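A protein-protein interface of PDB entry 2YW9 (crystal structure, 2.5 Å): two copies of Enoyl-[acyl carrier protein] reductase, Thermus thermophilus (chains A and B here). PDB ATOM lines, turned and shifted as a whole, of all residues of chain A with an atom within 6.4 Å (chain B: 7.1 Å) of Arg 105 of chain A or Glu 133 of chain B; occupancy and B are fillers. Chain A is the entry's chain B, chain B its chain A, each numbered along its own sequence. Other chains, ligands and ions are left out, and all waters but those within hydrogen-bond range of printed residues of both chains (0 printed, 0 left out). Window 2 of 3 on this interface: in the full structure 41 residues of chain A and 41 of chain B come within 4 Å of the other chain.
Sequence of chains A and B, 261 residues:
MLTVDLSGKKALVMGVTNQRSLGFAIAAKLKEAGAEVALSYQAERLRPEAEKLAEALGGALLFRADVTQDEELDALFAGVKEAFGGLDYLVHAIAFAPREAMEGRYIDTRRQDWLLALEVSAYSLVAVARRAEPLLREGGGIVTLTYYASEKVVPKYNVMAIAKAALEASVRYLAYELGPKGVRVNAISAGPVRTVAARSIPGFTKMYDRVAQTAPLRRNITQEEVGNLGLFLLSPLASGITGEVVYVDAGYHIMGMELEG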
ATOM      1  N   GLU A 100      14.365  26.384  -6.704  1.00  0.00           N
ATOM      2  CA  GLU A 100      12.930  26.270  -6.428  1.00  0.00           C
ATOM      3  C   GLU A 100      12.650  25.962  -4.954  1.00  0.00           C
ATOM      4  O   GLU A 100      11.621  26.372  -4.408  1.00  0.00           O
ATOM      5  CB  GLU A 100      12.273  25.217  -7.333  1.00  0.00           C
ATOM      6  N   ALA A 101      13.569  25.239  -4.317  1.00  0.00           N
ATOM      7  CA  ALA A 101      13.420  24.879  -2.910  1.00  0.00           C
ATOM      8  C   ALA A 101      13.648  26.091  -2.025  1.00  0.00           C
ATOM      9  O   ALA A 101      13.013  26.237  -0.986  1.00  0.00           O
ATOM     10  CB  ALA A 101      14.384  23.759  -2.540  1.00  0.00           C
ATOM     11  N   GLU A 103      13.070  29.194  -2.903  1.00  0.00           N
ATOM     12  CA  GLU A 103      12.001  30.170  -3.111  1.00  0.00           C
ATOM     13  C   GLU A 103      10.682  29.635  -2.572  1.00  0.00           C
ATOM     14  O   GLU A 103      10.288  28.505  -2.873  1.00  0.00           O
ATOM     15  CB  GLU A 103      11.848  30.510  -4.589  1.00  0.00           C
ATOM     16  CG  GLU A 103      13.006  31.297  -5.175  1.00  0.00           C
ATOM     17  CD  GLU A 103      12.869  31.458  -6.675  1.00  0.00           C
ATOM     18  OE1 GLU A 103      11.772  31.853  -7.124  1.00  0.00           O
ATOM     19  OE2 GLU A 103      13.850  31.185  -7.403  1.00  0.00           O
ATOM     20  N   GLY A 104      10.003  30.452  -1.771  1.00  0.00           N
ATOM     21  CA  GLY A 104       8.754  30.038  -1.132  1.00  0.00           C
ATOM     22  C   GLY A 104       8.950  29.425   0.244  1.00  0.00           C
ATOM     23  O   GLY A 104       9.919  29.741   0.942  1.00  0.00           O
ATOM     24  N   ARG A 105       8.029  28.543   0.628  1.00  0.00           N
ATOM     25  CA  ARG A 105       8.024  27.955   1.971  1.00  0.00           C
ATOM     26  C   ARG A 105       8.693  26.586   2.002  1.00  0.00           C
ATOM     27  O   ARG A 105       8.648  25.840   1.022  1.00  0.00           O
ATOM     28  CB  ARG A 105       6.597  27.809   2.493  1.00  0.00           C
ATOM     29  CG  ARG A 105       5.722  29.021   2.304  1.00  0.00           C
ATOM     30  CD  ARG A 105       4.328  28.569   1.896  1.00  0.00           C
ATOM     31  NE  ARG A 105       3.459  28.356   3.045  1.00  0.00           N
ATOM     32  CZ  ARG A 105       2.477  27.464   3.088  1.00  0.00           C
ATOM     33  NH1 ARG A 105       2.249  26.665   2.057  1.00  0.00           N
ATOM     34  NH2 ARG A 105       1.736  27.369   4.179  1.00  0.00           N
ATOM     35  N   TYR A 106       9.289  26.264   3.145  1.00  0.00           N
ATOM     36  CA  TYR A 106       9.924  24.972   3.354  1.00  0.00           C
ATOM     37  C   TYR A 106       8.935  23.833   3.132  1.00  0.00           C
ATOM     38  O   TYR A 106       9.288  22.779   2.591  1.00  0.00           O
ATOM     39  CB  TYR A 106      10.521  24.886   4.769  1.00  0.00           C
ATOM     40  CG  TYR A 106      11.056  23.517   5.115  1.00  0.00           C
ATOM     41  CD1 TYR A 106      10.527  22.781   6.170  1.00  0.00           C
ATOM     42  CD2 TYR A 106      12.076  22.946   4.364  1.00  0.00           C
ATOM     43  CE1 TYR A 106      11.013  21.519   6.473  1.00  0.00           C
ATOM     44  CE2 TYR A 106      12.567  21.690   4.657  1.00  0.00           C
ATOM     45  CZ  TYR A 106      12.036  20.978   5.712  1.00  0.00           C
ATOM     46  OH  TYR A 106      12.538  19.724   5.996  1.00  0.00           O
ATOM     47  N   ILE A 107       7.692  24.054   3.554  1.00  0.00           N
ATOM     48  CA  ILE A 107       6.660  23.029   3.473  1.00  0.00           C
ATOM     49  C   ILE A 107       6.303  22.696   2.021  1.00  0.00           C
ATOM     50  O   ILE A 107       5.709  21.654   1.739  1.00  0.00           O
ATOM     51  CB  ILE A 107       5.409  23.437   4.279  1.00  0.00           C
ATOM     52  CG1 ILE A 107       4.438  22.265   4.402  1.00  0.00           C
ATOM     53  CG2 ILE A 107       4.744  24.675   3.678  1.00  0.00           C
ATOM     54  CD1 ILE A 107       3.337  22.508   5.400  1.00  0.00           C
ATOM     55  N   ASP A 108       6.705  23.571   1.103  1.00  0.00           N
ATOM     56  CA  ASP A 108       6.436  23.378  -0.323  1.00  0.00           C
ATOM     57  C   ASP A 108       7.604  22.760  -1.103  1.00  0.00           C
ATOM     58  O   ASP A 108       7.536  22.616  -2.324  1.00  0.00           O
ATOM     59  CB  ASP A 108       6.010  24.703  -0.967  1.00  0.00           C
ATOM     60  CG  ASP A 108       4.661  25.174  -0.476  1.00  0.00           C
ATOM     61  OD1 ASP A 108       3.766  24.331  -0.278  1.00  0.00           O
ATOM     62  OD2 ASP A 108       4.489  26.388  -0.282  1.00  0.00           O
ATOM     63  N   THR A 109       8.671  22.394  -0.399  1.00  0.00           N
ATOM     64  CA  THR A 109       9.832  21.792  -1.043  1.00  0.00           C
ATOM     65  C   THR A 109       9.426  20.498  -1.744  1.00  0.00           C
ATOM     66  O   THR A 109       8.752  19.652  -1.155  1.00  0.00           O
ATOM     67  CB  THR A 109      10.954  21.504  -0.030  1.00  0.00           C
ATOM     68  OG1 THR A 109      11.156  22.652   0.797  1.00  0.00           O
ATOM     69  CG2 THR A 109      12.253  21.177  -0.739  1.00  0.00           C
ATOM     70  N   ASN A 158      14.946  27.778   4.517  1.00  0.00           N
ATOM     71  CA  ASN A 158      14.304  26.544   4.089  1.00  0.00           C
ATOM     72  C   ASN A 158      15.135  25.279   4.286  1.00  0.00           C
ATOM     73  O   ASN A 158      15.689  25.052   5.365  1.00  0.00           O
ATOM     74  CB  ASN A 158      13.823  26.684   2.644  1.00  0.00           C
ATOM     75  CG  ASN A 158      12.789  27.791   2.482  1.00  0.00           C
ATOM     76  OD1 ASN A 158      12.373  28.406   3.463  1.00  0.00           O
ATOM     77  ND2 ASN A 158      12.367  28.043   1.243  1.00  0.00           N
ATOM     78  N   PHE B  77      -4.966  12.112   0.967  1.00  0.00           N
ATOM     79  CA  PHE B  77      -5.531  13.347   1.499  1.00  0.00           C
ATOM     80  C   PHE B  77      -6.838  13.749   0.831  1.00  0.00           C
ATOM     81  O   PHE B  77      -7.671  14.407   1.448  1.00  0.00           O
ATOM     82  CB  PHE B  77      -4.496  14.480   1.510  1.00  0.00           C
ATOM     83  CG  PHE B  77      -3.578  14.419   2.697  1.00  0.00           C
ATOM     84  CD1 PHE B  77      -3.914  15.056   3.889  1.00  0.00           C
ATOM     85  CD2 PHE B  77      -2.405  13.672   2.649  1.00  0.00           C
ATOM     86  CE1 PHE B  77      -3.089  14.971   4.992  1.00  0.00           C
ATOM     87  CE2 PHE B  77      -1.569  13.589   3.747  1.00  0.00           C
ATOM     88  CZ  PHE B  77      -1.913  14.239   4.922  1.00  0.00           C
ATOM     89  N   LEU B  87      -9.514  18.126   8.917  1.00  0.00           N
ATOM     90  CA  LEU B  87      -8.634  17.347   9.772  1.00  0.00           C
ATOM     91  C   LEU B  87      -8.224  18.173  10.992  1.00  0.00           C
ATOM     92  O   LEU B  87      -8.041  19.389  10.900  1.00  0.00           O
ATOM     93  CB  LEU B  87      -7.406  16.884   8.988  1.00  0.00           C
ATOM     94  CG  LEU B  87      -6.490  15.813   9.594  1.00  0.00           C
ATOM     95  CD1 LEU B  87      -7.226  14.507   9.844  1.00  0.00           C
ATOM     96  CD2 LEU B  87      -5.295  15.571   8.682  1.00  0.00           C
ATOM     97  N   VAL B 126       7.372  16.751   5.833  1.00  0.00           N
ATOM     98  CA  VAL B 126       7.116  17.909   4.985  1.00  0.00           C
ATOM     99  C   VAL B 126       5.978  17.596   4.011  1.00  0.00           C
ATOM    100  O   VAL B 126       5.038  18.374   3.870  1.00  0.00           O
ATOM    101  CB  VAL B 126       8.383  18.306   4.200  1.00  0.00           C
ATOM    102  CG1 VAL B 126       8.137  19.531   3.329  1.00  0.00           C
ATOM    103  CG2 VAL B 126       9.543  18.541   5.160  1.00  0.00           C
ATOM    104  N   VAL B 128       3.531  15.333   4.069  1.00  0.00           N
ATOM    105  CA  VAL B 128       2.189  15.174   4.636  1.00  0.00           C
ATOM    106  C   VAL B 128       1.683  16.456   5.283  1.00  0.00           C
ATOM    107  O   VAL B 128       0.475  16.660   5.395  1.00  0.00           O
ATOM    108  CB  VAL B 128       2.104  13.998   5.629  1.00  0.00           C
ATOM    109  CG1 VAL B 128       2.574  12.724   4.961  1.00  0.00           C
ATOM    110  CG2 VAL B 128       2.919  14.279   6.884  1.00  0.00           C
ATOM    111  N   ALA B 129       2.604  17.321   5.699  1.00  0.00           N
ATOM    112  CA  ALA B 129       2.230  18.606   6.284  1.00  0.00           C
ATOM    113  C   ALA B 129       1.644  19.534   5.220  1.00  0.00           C
ATOM    114  O   ALA B 129       0.645  20.220   5.464  1.00  0.00           O
ATOM    115  CB  ALA B 129       3.430  19.265   6.969  1.00  0.00           C
ATOM    116  N   ARG B 130       2.265  19.546   4.042  1.00  0.00           N
ATOM    117  CA  ARG B 130       1.804  20.382   2.941  1.00  0.00           C
ATOM    118  C   ARG B 130       0.384  20.007   2.537  1.00  0.00           C
ATOM    119  O   ARG B 130      -0.471  20.873   2.315  1.00  0.00           O
ATOM    120  CB  ARG B 130       2.730  20.265   1.729  1.00  0.00           C
ATOM    121  CG  ARG B 130       2.396  21.286   0.667  1.00  0.00           C
ATOM    122  CD  ARG B 130       3.199  21.108  -0.594  1.00  0.00           C
ATOM    123  NE  ARG B 130       2.534  20.225  -1.543  1.00  0.00           N
ATOM    124  CZ  ARG B 130       3.120  19.183  -2.119  1.00  0.00           C
ATOM    125  NH1 ARG B 130       4.386  18.898  -1.839  1.00  0.00           N
ATOM    126  NH2 ARG B 130       2.440  18.436  -2.985  1.00  0.00           N
ATOM    127  N   ARG B 131       0.144  18.706   2.456  1.00  0.00           N
ATOM    128  CA  ARG B 131      -1.148  18.200   2.054  1.00  0.00           C
ATOM    129  C   ARG B 131      -2.192  18.307   3.168  1.00  0.00           C
ATOM    130  O   ARG B 131      -3.382  18.411   2.891  1.00  0.00           O
ATOM    131  CB  ARG B 131      -1.000  16.765   1.554  1.00  0.00           C
ATOM    132  CG  ARG B 131      -0.188  16.689   0.263  1.00  0.00           C
ATOM    133  CD  ARG B 131       0.220  15.275  -0.065  1.00  0.00           C
ATOM    134  NE  ARG B 131       0.870  15.179  -1.371  1.00  0.00           N
ATOM    135  CZ  ARG B 131       2.146  15.479  -1.602  1.00  0.00           C
ATOM    136  NH1 ARG B 131       2.929  15.911  -0.620  1.00  0.00           N
ATOM    137  NH2 ARG B 131       2.647  15.348  -2.822  1.00  0.00           N
ATOM    138  N   ALA B 132      -1.747  18.305   4.421  1.00  0.00           N
ATOM    139  CA  ALA B 132      -2.677  18.453   5.541  1.00  0.00           C
ATOM    140  C   ALA B 132      -3.055  19.909   5.754  1.00  0.00           C
ATOM    141  O   ALA B 132      -4.145  20.206   6.235  1.00  0.00           O
ATOM    142  CB  ALA B 132      -2.091  17.861   6.823  1.00  0.00           C
ATOM    143  N   GLU B 133      -2.159  20.818   5.383  1.00  0.00           N
ATOM    144  CA  GLU B 133      -2.384  22.244   5.637  1.00  0.00           C
ATOM    145  C   GLU B 133      -3.774  22.793   5.258  1.00  0.00           C
ATOM    146  O   GLU B 133      -4.421  23.443   6.082  1.00  0.00           O
ATOM    147  CB  GLU B 133      -1.278  23.102   5.019  1.00  0.00           C
ATOM    148  CG  GLU B 133      -1.500  24.579   5.255  1.00  0.00           C
ATOM    149  CD  GLU B 133      -0.455  25.446   4.602  1.00  0.00           C
ATOM    150  OE1 GLU B 133      -0.264  26.582   5.083  1.00  0.00           O
ATOM    151  OE2 GLU B 133       0.176  24.997   3.618  1.00  0.00           O
ATOM    152  N   PRO B 134      -4.247  22.526   4.020  1.00  0.00           N
ATOM    153  CA  PRO B 134      -5.578  23.040   3.665  1.00  0.00           C
ATOM    154  C   PRO B 134      -6.742  22.325   4.377  1.00  0.00           C
ATOM    155  O   PRO B 134      -7.855  22.855   4.408  1.00  0.00           O
ATOM    156  CB  PRO B 134      -5.662  22.815   2.144  1.00  0.00           C
ATOM    157  CG  PRO B 134      -4.297  22.357   1.711  1.00  0.00           C
ATOM    158  CD  PRO B 134      -3.635  21.777   2.908  1.00  0.00           C
ATOM    159  N   LEU B 135      -6.487  21.145   4.942  1.00  0.00           N
ATOM    160  CA  LEU B 135      -7.519  20.396   5.667  1.00  0.00           C
ATOM    161  C   LEU B 135      -7.571  20.747   7.154  1.00  0.00           C
ATOM    162  O   LEU B 135      -8.595  20.549   7.813  1.00  0.00           O
ATOM    163  CB  LEU B 135      -7.288  18.890   5.524  1.00  0.00           C
ATOM    164  CG  LEU B 135      -7.325  18.274   4.123  1.00  0.00           C
ATOM    165  CD1 LEU B 135      -7.350  16.762   4.234  1.00  0.00           C
ATOM    166  CD2 LEU B 135      -8.530  18.771   3.314  1.00  0.00           C
ATOM    167  N   LEU B 136      -6.462  21.264   7.678  1.00  0.00           N
ATOM    168  CA  LEU B 136      -6.312  21.477   9.115  1.00  0.00           C
ATOM    169  C   LEU B 136      -7.097  22.664   9.674  1.00  0.00           C
ATOM    170  O   LEU B 136      -6.974  23.793   9.196  1.00  0.00           O
ATOM    171  CB  LEU B 136      -4.835  21.589   9.475  1.00  0.00           C
ATOM    172  CG  LEU B 136      -4.076  20.261   9.481  1.00  0.00           C
ATOM    173  CD1 LEU B 136      -2.581  20.520   9.497  1.00  0.00           C
ATOM    174  CD2 LEU B 136      -4.497  19.392  10.663  1.00  0.00           C
ATOM    175  N   ARG B 137      -7.901  22.397  10.696  1.00  0.00           N
ATOM    176  CA  ARG B 137      -8.747  23.419  11.297  1.00  0.00           C
ATOM    177  C   ARG B 137      -7.991  24.153  12.398  1.00  0.00           C
ATOM    178  O   ARG B 137      -6.952  23.685  12.860  1.00  0.00           O
ATOM    179  CB  ARG B 137     -10.015  22.793  11.881  1.00  0.00           C
ATOM    180  CG  ARG B 137     -10.758  21.846  10.939  1.00  0.00           C
ATOM    181  CD  ARG B 137     -11.627  20.866  11.721  1.00  0.00           C
ATOM    182  NE  ARG B 137     -12.447  20.037  10.836  1.00  0.00           N
ATOM    183  CZ  ARG B 137     -13.231  19.041  11.248  1.00  0.00           C
ATOM    184  NH1 ARG B 137     -13.312  18.731  12.540  1.00  0.00           N
ATOM    185  NH2 ARG B 137     -13.937  18.349  10.361  1.00  0.00           N
ATOM    186  N   ILE B 142       0.106  18.872  14.473  1.00  0.00           N
ATOM    187  CA  ILE B 142       0.907  17.791  13.925  1.00  0.00           C
ATOM    188  C   ILE B 142       1.929  17.358  14.976  1.00  0.00           C
ATOM    189  O   ILE B 142       2.571  18.189  15.619  1.00  0.00           O
ATOM    190  CB  ILE B 142       1.634  18.223  12.622  1.00  0.00           C
ATOM    191  CG1 ILE B 142       0.627  18.730  11.580  1.00  0.00           C
ATOM    192  CG2 ILE B 142       2.450  17.077  12.051  1.00  0.00           C
ATOM    193  CD1 ILE B 142       1.261  19.216  10.283  1.00  0.00           C
ATOM    194  N   GLU B 177       5.792  28.158   9.861  1.00  0.00           N
ATOM    195  CA  GLU B 177       5.001  28.378   8.657  1.00  0.00           C
ATOM    196  C   GLU B 177       3.513  28.045   8.827  1.00  0.00           C
ATOM    197  O   GLU B 177       2.665  28.694   8.228  1.00  0.00           O
ATOM    198  CB  GLU B 177       5.606  27.617   7.474  1.00  0.00           C
ATOM    199  CG  GLU B 177       7.006  28.096   7.092  1.00  0.00           C
ATOM    200  CD  GLU B 177       7.590  27.356   5.903  1.00  0.00           C
ATOM    201  OE1 GLU B 177       8.539  27.880   5.289  1.00  0.00           O
ATOM    202  OE2 GLU B 177       7.114  26.248   5.575  1.00  0.00           O
ATOM    203  N   LEU B 178       3.190  27.044   9.642  1.00  0.00           N
ATOM    204  CA  LEU B 178       1.793  26.650   9.851  1.00  0.00           C
ATOM    205  C   LEU B 178       1.141  27.334  11.058  1.00  0.00           C
ATOM    206  O   LEU B 178      -0.070  27.227  11.268  1.00  0.00           O
ATOM    207  CB  LEU B 178       1.676  25.132   9.991  1.00  0.00           C
ATOM    208  CG  LEU B 178       2.178  24.287   8.822  1.00  0.00           C
ATOM    209  CD1 LEU B 178       1.890  22.817   9.078  1.00  0.00           C
ATOM    210  CD2 LEU B 178       1.540  24.749   7.519  1.00  0.00           C
ATOM    211  N   LYS B 181      -1.959  30.063  10.870  1.00  0.00           N
ATOM    212  CA  LYS B 181      -3.278  29.481  10.624  1.00  0.00           C
ATOM    213  C   LYS B 181      -3.784  28.657  11.810  1.00  0.00           C
ATOM    214  O   LYS B 181      -4.722  27.867  11.671  1.00  0.00           O
ATOM    215  CB  LYS B 181      -3.266  28.620   9.353  1.00  0.00           C
ATOM    216  N   VAL B 183      -2.224  26.240  13.511  1.00  0.00           N
ATOM    217  CA  VAL B 183      -1.734  24.868  13.564  1.00  0.00           C
ATOM    218  C   VAL B 183      -0.414  24.796  14.327  1.00  0.00           C
ATOM    219  O   VAL B 183       0.508  25.568  14.069  1.00  0.00           O
ATOM    220  CB  VAL B 183      -1.537  24.287  12.146  1.00  0.00           C
ATOM    221  CG1 VAL B 183      -1.098  22.828  12.223  1.00  0.00           C
ATOM    222  CG2 VAL B 183      -2.824  24.423  11.335  1.00  0.00           C
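The side-chain carboxylate of Glu 177 of chain B lies within hydrogen-bond range of the backbone NH of Tyr 106 of chain A. The side-chain carboxylate (OE2) of Glu 133 of chain B lies within salt-bridge range of the guanidinium group (NH2) of Arg 105 of chain A, at 2.9 Å. The side-chain carboxylate (OE2) of Glu 177 of chain B is in hydrogen-bond range of the backbone NH (N) of Ile 107 of chain A, at 3.0 Å.
O of Tyr 106 of chain A is in hydrogen-bond range of OG1 of Thr 109 of chain A (2.6 Å). The backbone NH of Val 183 of chain B sits at hydrogen-bond distance from the backbone carbonyl oxygen of Leu 178 of chain B, 3.3 Å away. The guanidinium group (NH1) of Arg 105 of chain A is in salt-bridge range of the side-chain carboxylate (OD2) of Asp 108 of chain A, at 3.3 Å.
Arg 105 of chain A touches Glu 177 of chain B (CA to OE1, 3.4 Å). OH of Tyr 106 of chain A touches CG2 of Val 126 of chain B, at 3.3 Å. Ile 107 of chain A touches Val 126 of chain B. Ile 107 of chain A touches Ala 129 of chain B (CD1 to C, 3.4 Å). CB of Arg 130 of chain B touches O of Ile 107 of chain A, at 3.3 Å. Ile 107 of chain A touches Leu 178 of chain B (CD1 to CD2, 3.6 Å). Arg 130 of chain B touches Asp 108 of chain A.
Arg 105 of chain A touches just these residues of chain B: Glu 133 and Glu 177. Printed residues of chain A within 4 Å of Arg 130 of chain B: Ile 107 and Asp 108. Glu 133 of chain B touches one residue of chain A. Printed residues of chain A within 4 Å of Leu 178 of chain B: Ile 107 (3.6 Å). The nearest residue of chain B that does not touch Arg 105 of chain A is Leu 178 of chain B (4.2 Å). The nearest printed residue of chain A that does not touch Glu 177 of chain B is Asn 158 of chain A (4.3 Å).
Hydrophobic or aromatic side chains of chain A that line the printed part of chain B: Tyr 106 and Ile 107. Printed residues of chain B that touch a printed residue of chain A: Val 126, Ala 129, Arg 130, Glu 133, Glu 177 and Leu 178. Hydrophobic or aromatic side chains of chain B that line the printed part of chain A: Val 126, Ala 129 and Leu 178. Among the printed residues, Asp or Glu carboxylates within 4 Å of a Lys or Arg side-chain nitrogen of the other chain: Arg 105 of chain A with Glu 133 of chain B.
No position is printed for both chains. Of the 10 pairs that touch across the chains among the printed residues, none has its exchanged pair printed and touching as well.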
